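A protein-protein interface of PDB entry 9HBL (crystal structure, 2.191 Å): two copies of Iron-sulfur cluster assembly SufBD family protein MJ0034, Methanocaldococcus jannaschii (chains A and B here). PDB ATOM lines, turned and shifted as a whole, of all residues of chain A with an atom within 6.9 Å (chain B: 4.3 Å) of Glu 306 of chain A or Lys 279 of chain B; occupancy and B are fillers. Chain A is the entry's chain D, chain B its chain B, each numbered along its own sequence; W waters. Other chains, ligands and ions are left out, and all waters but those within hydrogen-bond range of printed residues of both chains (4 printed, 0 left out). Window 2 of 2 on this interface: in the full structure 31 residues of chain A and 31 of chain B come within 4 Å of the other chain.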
ATOM      1  N   VAL A 261      -0.700 -20.632  36.489  1.00  0.00           N
ATOM      2  CA  VAL A 261      -1.074 -19.325  35.959  1.00  0.00           C
ATOM      3  C   VAL A 261      -1.359 -19.490  34.452  1.00  0.00           C
ATOM      4  O   VAL A 261      -0.525 -20.012  33.713  1.00  0.00           O
ATOM      5  CB  VAL A 261       0.028 -18.271  36.197  1.00  0.00           C
ATOM      6  CG1 VAL A 261      -0.308 -16.958  35.503  1.00  0.00           C
ATOM      7  CG2 VAL A 261       0.277 -18.061  37.678  1.00  0.00           C
ATOM      8  N   LYS A 262      -2.540 -19.060  34.018  1.00  0.00           N
ATOM      9  CA  LYS A 262      -2.964 -19.077  32.618  1.00  0.00           C
ATOM     10  C   LYS A 262      -3.541 -17.679  32.295  1.00  0.00           C
ATOM     11  O   LYS A 262      -4.087 -17.010  33.182  1.00  0.00           O
ATOM     12  CB  LYS A 262      -4.032 -20.158  32.407  1.00  0.00           C
ATOM     13  CG  LYS A 262      -3.489 -21.443  31.817  1.00  0.00           C
ATOM     14  CD  LYS A 262      -3.141 -21.228  30.327  1.00  0.00           C
ATOM     15  CE  LYS A 262      -2.247 -22.284  29.734  1.00  0.00           C
ATOM     16  NZ  LYS A 262      -0.926 -21.732  29.338  1.00  0.00           N
ATOM     17  N   GLY A 263      -3.417 -17.246  31.050  1.00  0.00           N
ATOM     18  CA  GLY A 263      -3.919 -15.941  30.640  1.00  0.00           C
ATOM     19  C   GLY A 263      -3.206 -14.793  31.313  1.00  0.00           C
ATOM     20  O   GLY A 263      -1.988 -14.842  31.484  1.00  0.00           O
ATOM     21  N   GLY A 289       3.320 -20.448  38.554  1.00  0.00           N
ATOM     22  CA  GLY A 289       3.497 -20.116  37.145  1.00  0.00           C
ATOM     23  C   GLY A 289       2.970 -21.151  36.189  1.00  0.00           C
ATOM     24  O   GLY A 289       1.947 -21.783  36.450  1.00  0.00           O
ATOM     25  N   SER A 290       3.647 -21.318  35.060  1.00  0.00           N
ATOM     26  CA  SER A 290       3.238 -22.285  34.044  1.00  0.00           C
ATOM     27  C   SER A 290       3.358 -23.716  34.533  1.00  0.00           C
ATOM     28  O   SER A 290       4.088 -23.983  35.484  1.00  0.00           O
ATOM     29  CB  SER A 290       4.076 -22.107  32.784  1.00  0.00           C
ATOM     30  OG  SER A 290       5.431 -22.379  33.070  1.00  0.00           O
ATOM     31  N   VAL A 291       2.643 -24.655  33.886  1.00  0.00           N
ATOM     32  CA  VAL A 291       2.714 -26.070  34.290  1.00  0.00           C
ATOM     33  C   VAL A 291       4.131 -26.606  34.161  1.00  0.00           C
ATOM     34  O   VAL A 291       4.885 -26.132  33.312  1.00  0.00           O
ATOM     35  CB  VAL A 291       1.681 -26.960  33.547  1.00  0.00           C
ATOM     36  CG1 VAL A 291       0.259 -26.435  33.756  1.00  0.00           C
ATOM     37  CG2 VAL A 291       2.004 -27.057  32.063  1.00  0.00           C
ATOM     38  N   LEU A 296       4.079 -31.725  31.315  1.00  0.00           N
ATOM     39  CA  LEU A 296       3.472 -31.341  30.061  1.00  0.00           C
ATOM     40  C   LEU A 296       4.009 -32.237  28.961  1.00  0.00           C
ATOM     41  O   LEU A 296       3.219 -32.849  28.251  1.00  0.00           O
ATOM     42  CB  LEU A 296       3.792 -29.868  29.785  1.00  0.00           C
ATOM     43  CG  LEU A 296       3.256 -29.301  28.507  1.00  0.00           C
ATOM     44  CD1 LEU A 296       1.749 -29.256  28.529  1.00  0.00           C
ATOM     45  CD2 LEU A 296       3.821 -27.934  28.257  1.00  0.00           C
ATOM     46  N   MET A 300       2.284 -35.005  26.445  1.00  0.00           N
ATOM     47  CA  MET A 300       2.396 -34.825  25.001  1.00  0.00           C
ATOM     48  C   MET A 300       3.038 -36.037  24.306  1.00  0.00           C
ATOM     49  O   MET A 300       2.760 -36.281  23.132  1.00  0.00           O
ATOM     50  CB  MET A 300       3.140 -33.541  24.673  1.00  0.00           C
ATOM     51  CG  MET A 300       2.503 -32.332  25.316  1.00  0.00           C
ATOM     52  SD  MET A 300       3.111 -30.766  24.669  1.00  0.00           S
ATOM     53  CE  MET A 300       4.777 -30.866  25.040  1.00  0.00           C
ATOM     54  N   LEU A 304      -1.251 -36.362  23.363  1.00  0.00           N
ATOM     55  CA  LEU A 304      -2.117 -35.229  23.706  1.00  0.00           C
ATOM     56  C   LEU A 304      -1.461 -33.939  23.221  1.00  0.00           C
ATOM     57  O   LEU A 304      -0.234 -33.827  23.299  1.00  0.00           O
ATOM     58  CB  LEU A 304      -2.290 -35.125  25.215  1.00  0.00           C
ATOM     59  CG  LEU A 304      -3.237 -36.082  25.887  1.00  0.00           C
ATOM     60  CD1 LEU A 304      -3.099 -35.949  27.350  1.00  0.00           C
ATOM     61  CD2 LEU A 304      -4.671 -35.830  25.517  1.00  0.00           C
ATOM     62  N   ASP A 305      -2.246 -32.953  22.730  1.00  0.00           N
ATOM     63  CA  ASP A 305      -1.631 -31.669  22.346  1.00  0.00           C
ATOM     64  C   ASP A 305      -1.360 -30.814  23.596  1.00  0.00           C
ATOM     65  O   ASP A 305      -1.872 -31.131  24.671  1.00  0.00           O
ATOM     66  CB  ASP A 305      -2.391 -30.914  21.230  1.00  0.00           C
ATOM     67  CG  ASP A 305      -3.781 -30.398  21.541  1.00  0.00           C
ATOM     68  OD1 ASP A 305      -3.996 -29.898  22.666  1.00  0.00           O
ATOM     69  OD2 ASP A 305      -4.638 -30.445  20.641  1.00  0.00           O
ATOM     70  N   GLU A 306      -0.568 -29.738  23.469  1.00  0.00           N
ATOM     71  CA  GLU A 306      -0.262 -28.858  24.600  1.00  0.00           C
ATOM     72  C   GLU A 306      -1.486 -28.371  25.359  1.00  0.00           C
ATOM     73  O   GLU A 306      -1.440 -28.267  26.581  1.00  0.00           O
ATOM     74  CB  GLU A 306       0.576 -27.673  24.136  1.00  0.00           C
ATOM     75  CG  GLU A 306       1.080 -26.807  25.271  1.00  0.00           C
ATOM     76  CD  GLU A 306       2.233 -25.895  24.908  1.00  0.00           C
ATOM     77  OE1 GLU A 306       2.782 -26.034  23.793  1.00  0.00           O
ATOM     78  OE2 GLU A 306       2.599 -25.048  25.751  1.00  0.00           O
ATOM     79  N   ASP A 307      -2.589 -28.089  24.657  1.00  0.00           N
ATOM     80  CA  ASP A 307      -3.811 -27.623  25.320  1.00  0.00           C
ATOM     81  C   ASP A 307      -4.545 -28.742  26.034  1.00  0.00           C
ATOM     82  O   ASP A 307      -5.045 -28.522  27.119  1.00  0.00           O
ATOM     83  CB  ASP A 307      -4.730 -26.879  24.344  1.00  0.00           C
ATOM     84  CG  ASP A 307      -4.125 -25.577  23.853  1.00  0.00           C
ATOM     85  OD1 ASP A 307      -3.539 -24.844  24.685  1.00  0.00           O
ATOM     86  OD2 ASP A 307      -4.211 -25.303  22.630  1.00  0.00           O
ATOM     87  N   GLU A 308      -4.586 -29.949  25.454  1.00  0.00           N
ATOM     88  CA  GLU A 308      -5.230 -31.090  26.101  1.00  0.00           C
ATOM     89  C   GLU A 308      -4.436 -31.478  27.348  1.00  0.00           C
ATOM     90  O   GLU A 308      -5.033 -31.734  28.386  1.00  0.00           O
ATOM     91  CB  GLU A 308      -5.315 -32.292  25.141  1.00  0.00           C
ATOM     92  CG  GLU A 308      -6.251 -32.090  23.965  1.00  0.00           C
ATOM     93  CD  GLU A 308      -6.053 -33.034  22.798  1.00  0.00           C
ATOM     94  OE1 GLU A 308      -5.008 -33.720  22.755  1.00  0.00           O
ATOM     95  OE2 GLU A 308      -6.934 -33.065  21.910  1.00  0.00           O
ATOM     96  N   ALA A 309      -3.089 -31.499  27.245  1.00  0.00           N
ATOM     97  CA  ALA A 309      -2.175 -31.852  28.332  1.00  0.00           C
ATOM     98  C   ALA A 309      -2.271 -30.863  29.490  1.00  0.00           C
ATOM     99  O   ALA A 309      -2.310 -31.285  30.651  1.00  0.00           O
ATOM    100  CB  ALA A 309      -0.749 -31.918  27.816  1.00  0.00           C
ATOM    101  N   THR A 310      -2.339 -29.548  29.177  1.00  0.00           N
ATOM    102  CA  THR A 310      -2.464 -28.494  30.182  1.00  0.00           C
ATOM    103  C   THR A 310      -3.811 -28.623  30.890  1.00  0.00           C
ATOM    104  O   THR A 310      -3.865 -28.570  32.112  1.00  0.00           O
ATOM    105  CB  THR A 310      -2.276 -27.115  29.534  1.00  0.00           C
ATOM    106  OG1 THR A 310      -0.979 -27.031  28.937  1.00  0.00           O
ATOM    107  CG2 THR A 310      -2.466 -25.984  30.508  1.00  0.00           C
ATOM    108  N   GLU A 311      -4.885 -28.851  30.126  1.00  0.00           N
ATOM    109  CA  GLU A 311      -6.233 -29.056  30.646  1.00  0.00           C
ATOM    110  C   GLU A 311      -6.282 -30.246  31.617  1.00  0.00           C
ATOM    111  O   GLU A 311      -6.944 -30.148  32.629  1.00  0.00           O
ATOM    112  CB  GLU A 311      -7.200 -29.278  29.479  1.00  0.00           C
ATOM    113  CG  GLU A 311      -8.677 -29.115  29.803  1.00  0.00           C
ATOM    114  CD  GLU A 311      -9.615 -29.681  28.743  1.00  0.00           C
ATOM    115  OE1 GLU A 311     -10.847 -29.667  28.977  1.00  0.00           O
ATOM    116  OE2 GLU A 311      -9.126 -30.147  27.686  1.00  0.00           O
ATOM    117  N   PRO B 249       7.410 -13.446  29.711  1.00  0.00           N
ATOM    118  CA  PRO B 249       7.370 -14.836  29.245  1.00  0.00           C
ATOM    119  C   PRO B 249       8.746 -15.469  29.256  1.00  0.00           C
ATOM    120  O   PRO B 249       9.740 -14.797  28.966  1.00  0.00           O
ATOM    121  CB  PRO B 249       6.816 -14.731  27.827  1.00  0.00           C
ATOM    122  CG  PRO B 249       7.112 -13.315  27.403  1.00  0.00           C
ATOM    123  CD  PRO B 249       7.040 -12.493  28.641  1.00  0.00           C
ATOM    124  N   TYR B 250       8.792 -16.735  29.699  1.00  0.00           N
ATOM    125  CA  TYR B 250       9.964 -17.580  29.804  1.00  0.00           C
ATOM    126  C   TYR B 250      10.948 -17.156  30.904  1.00  0.00           C
ATOM    127  O   TYR B 250      12.041 -17.725  30.984  1.00  0.00           O
ATOM    128  CB  TYR B 250      10.641 -17.753  28.444  1.00  0.00           C
ATOM    129  CG  TYR B 250       9.660 -18.320  27.443  1.00  0.00           C
ATOM    130  CD1 TYR B 250       9.096 -19.573  27.634  1.00  0.00           C
ATOM    131  CD2 TYR B 250       9.200 -17.555  26.378  1.00  0.00           C
ATOM    132  CE1 TYR B 250       8.157 -20.083  26.752  1.00  0.00           C
ATOM    133  CE2 TYR B 250       8.243 -18.045  25.499  1.00  0.00           C
ATOM    134  CZ  TYR B 250       7.735 -19.317  25.682  1.00  0.00           C
ATOM    135  OH  TYR B 250       6.799 -19.837  24.819  1.00  0.00           O
ATOM    136  N   SER B 251      10.531 -16.261  31.818  1.00  0.00           N
ATOM    137  CA  SER B 251      11.380 -15.897  32.954  1.00  0.00           C
ATOM    138  C   SER B 251      11.305 -17.025  33.991  1.00  0.00           C
ATOM    139  O   SER B 251      10.233 -17.593  34.214  1.00  0.00           O
ATOM    140  CB  SER B 251      10.964 -14.554  33.553  1.00  0.00           C
ATOM    141  OG  SER B 251       9.639 -14.591  34.047  1.00  0.00           O
ATOM    142  N   LYS B 252      12.448 -17.426  34.548  1.00  0.00           N
ATOM    143  CA  LYS B 252      12.487 -18.533  35.513  1.00  0.00           C
ATOM    144  C   LYS B 252      13.248 -18.104  36.755  1.00  0.00           C
ATOM    145  O   LYS B 252      14.250 -17.396  36.640  1.00  0.00           O
ATOM    146  CB  LYS B 252      13.171 -19.770  34.910  1.00  0.00           C
ATOM    147  CG  LYS B 252      12.478 -20.340  33.678  1.00  0.00           C
ATOM    148  CD  LYS B 252      11.049 -20.830  33.956  1.00  0.00           C
ATOM    149  CE  LYS B 252      10.349 -21.384  32.720  1.00  0.00           C
ATOM    150  NZ  LYS B 252       9.125 -20.610  32.352  1.00  0.00           N
ATOM    151  N   ASP B 277       2.904 -13.574  34.273  1.00  0.00           N
ATOM    152  CA  ASP B 277       2.933 -14.103  32.906  1.00  0.00           C
ATOM    153  C   ASP B 277       2.651 -15.615  32.934  1.00  0.00           C
ATOM    154  O   ASP B 277       3.183 -16.300  33.798  1.00  0.00           O
ATOM    155  CB  ASP B 277       4.270 -13.831  32.227  1.00  0.00           C
ATOM    156  CG  ASP B 277       4.167 -13.958  30.718  1.00  0.00           C
ATOM    157  OD1 ASP B 277       4.272 -15.094  30.207  1.00  0.00           O
ATOM    158  OD2 ASP B 277       3.961 -12.920  30.044  1.00  0.00           O
ATOM    159  N   ASP B 278       1.822 -16.139  32.007  1.00  0.00           N
ATOM    160  CA  ASP B 278       1.492 -17.566  32.000  1.00  0.00           C
ATOM    161  C   ASP B 278       2.626 -18.480  31.464  1.00  0.00           C
ATOM    162  O   ASP B 278       2.481 -19.704  31.496  1.00  0.00           O
ATOM    163  CB  ASP B 278       0.158 -17.851  31.273  1.00  0.00           C
ATOM    164  CG  ASP B 278       0.142 -17.726  29.761  1.00  0.00           C
ATOM    165  OD1 ASP B 278       1.141 -17.226  29.190  1.00  0.00           O
ATOM    166  OD2 ASP B 278      -0.869 -18.119  29.148  1.00  0.00           O
ATOM    167  N   LYS B 279       3.723 -17.880  30.943  1.00  0.00           N
ATOM    168  CA  LYS B 279       4.906 -18.612  30.476  1.00  0.00           C
ATOM    169  C   LYS B 279       6.108 -18.412  31.403  1.00  0.00           C
ATOM    170  O   LYS B 279       7.220 -18.758  31.015  1.00  0.00           O
ATOM    171  CB  LYS B 279       5.299 -18.228  29.033  1.00  0.00           C
ATOM    172  CG  LYS B 279       4.289 -18.631  27.955  1.00  0.00           C
ATOM    173  CD  LYS B 279       4.010 -20.154  27.933  1.00  0.00           C
ATOM    174  CE  LYS B 279       2.523 -20.448  27.945  1.00  0.00           C
ATOM    175  NZ  LYS B 279       2.237 -21.815  27.449  1.00  0.00           N
ATOM    176  N   ALA B 280       5.900 -17.858  32.611  1.00  0.00           N
ATOM    177  CA  ALA B 280       6.902 -17.620  33.654  1.00  0.00           C
ATOM    178  C   ALA B 280       6.739 -18.704  34.711  1.00  0.00           C
ATOM    179  O   ALA B 280       5.627 -19.211  34.890  1.00  0.00           O
ATOM    180  CB  ALA B 280       6.658 -16.250  34.291  1.00  0.00           C
HETATM  181  O   HOH W   1       6.851 -21.630  30.434  1.00  0.00           O
HETATM  182  O   HOH W   2       0.276 -14.176  30.129  1.00  0.00           O
HETATM  183  O   HOH W   3       0.382 -21.602  31.881  1.00  0.00           O
HETATM  184  O   HOH W   4       1.087 -24.710  28.900  1.00  0.00           O
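OD2 of Asp 278 of chain B is in salt-bridge range of NZ of Lys 262 of chain A, 3.6 Å away. OE2 of Glu 306 of chain A lies within salt-bridge range of NZ of Lys 279 of chain B. The backbone carbonyl oxygen (O) of Ala 280 of chain B sits at hydrogen-bond distance from the backbone NH (N) of Ser 290 of chain A, at 2.9 Å. The side-chain carboxylate (OD2) of Asp 278 of chain B sits at hydrogen-bond distance from the backbone NH (N) of Gly 263 of chain A (3.3 Å).
The side-chain carboxylate (OD1) of Asp 277 of chain B sits at hydrogen-bond distance from the backbone NH (N) of Lys 279 of chain B (2.9 Å). The backbone NH (N) of Tyr 250 of chain B is in hydrogen-bond range of the backbone carbonyl oxygen (O) of Lys 279 of chain B, 2.9 Å away. OG1 of Thr 310 of chain A lies within hydrogen-bond range of O of Glu 306 of chain A (2.7 Å). The backbone NH (N) of Val 261 of chain A lies within hydrogen-bond range of the backbone carbonyl oxygen (O) of Gly 289 of chain A (2.9 Å). The side-chain amino group of Lys 252 of chain B is in hydrogen-bond range of the backbone carbonyl oxygen of Lys 279 of chain B, 3.0 Å away.
Among the printed residues, pairs that only touch across the chains: Ser 290 of chain A with Asp 278 of chain B, Gly 289 of chain A with Ala 280 of chain B, Val 261 of chain A with Asp 278 of chain B, Lys 262 of chain A with Lys 279 of chain B and Val 261 of chain A with Asp 277 of chain B.
Met 300 of chain A touches none of the printed residues of chain B. Leu 304 of chain A touches none of the printed residues of chain B. Glu 306 of chain A touches just one residue of chain B: Lys 279 (3.7 Å). Printed residues of chain A within 4 Å of Asp 277 of chain B: Val 261. Printed residues of chain A within 4 Å of Asp 278 of chain B: Val 261, Lys 262, Gly 263 and Ser 290. Lys 279 of chain B touches just these residues of chain A: Lys 262 (3.7 Å) and Glu 306 (3.7 Å). The nearest printed residue of chain B that does not touch Glu 306 of chain A is Tyr 250 of chain B (6.8 Å).
Hydrophobic or aromatic side chains of chain A that line the printed part of chain B: Val 261. Printed residues of chain B that touch a printed residue of chain A: Asp 277, Asp 278, Lys 279 and Ala 280. Among the printed residues, Asp or Glu carboxylates within 4 Å of a Lys or Arg side-chain nitrogen of the other chain: Lys 262 of chain A with Asp 278 of chain B (3.6 Å) and Glu 306 of chain A with Lys 279 of chain B (3.7 Å).
No position is printed for both chains. Of the 9 pairs that touch across the chains among the printed residues, none has its exchanged pair printed and touching as well.
Water W3 lies within hydrogen-bond range of O of Val 261 of chain A (2.6 Å), O of Asp 278 of chain B (2.9 Å) and NZ of Lys 262 of chain A (2.9 Å). Water W2 bridges O of Gly 263 of chain A and N of Asp 278 of chain B. Water W1 lies within hydrogen-bond range of O of Lys 279 of chain B (3.0 Å), OG of Ser 290 of chain A (3.1 Å) and NZ of Lys 252 of chain B (3.1 Å). Water W4 bridges the side-chain hydroxyl (OG1) of Thr 310 of chain A (3.1 Å) and the side-chain amino group (NZ) of Lys 279 of chain B (3.4 Å).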
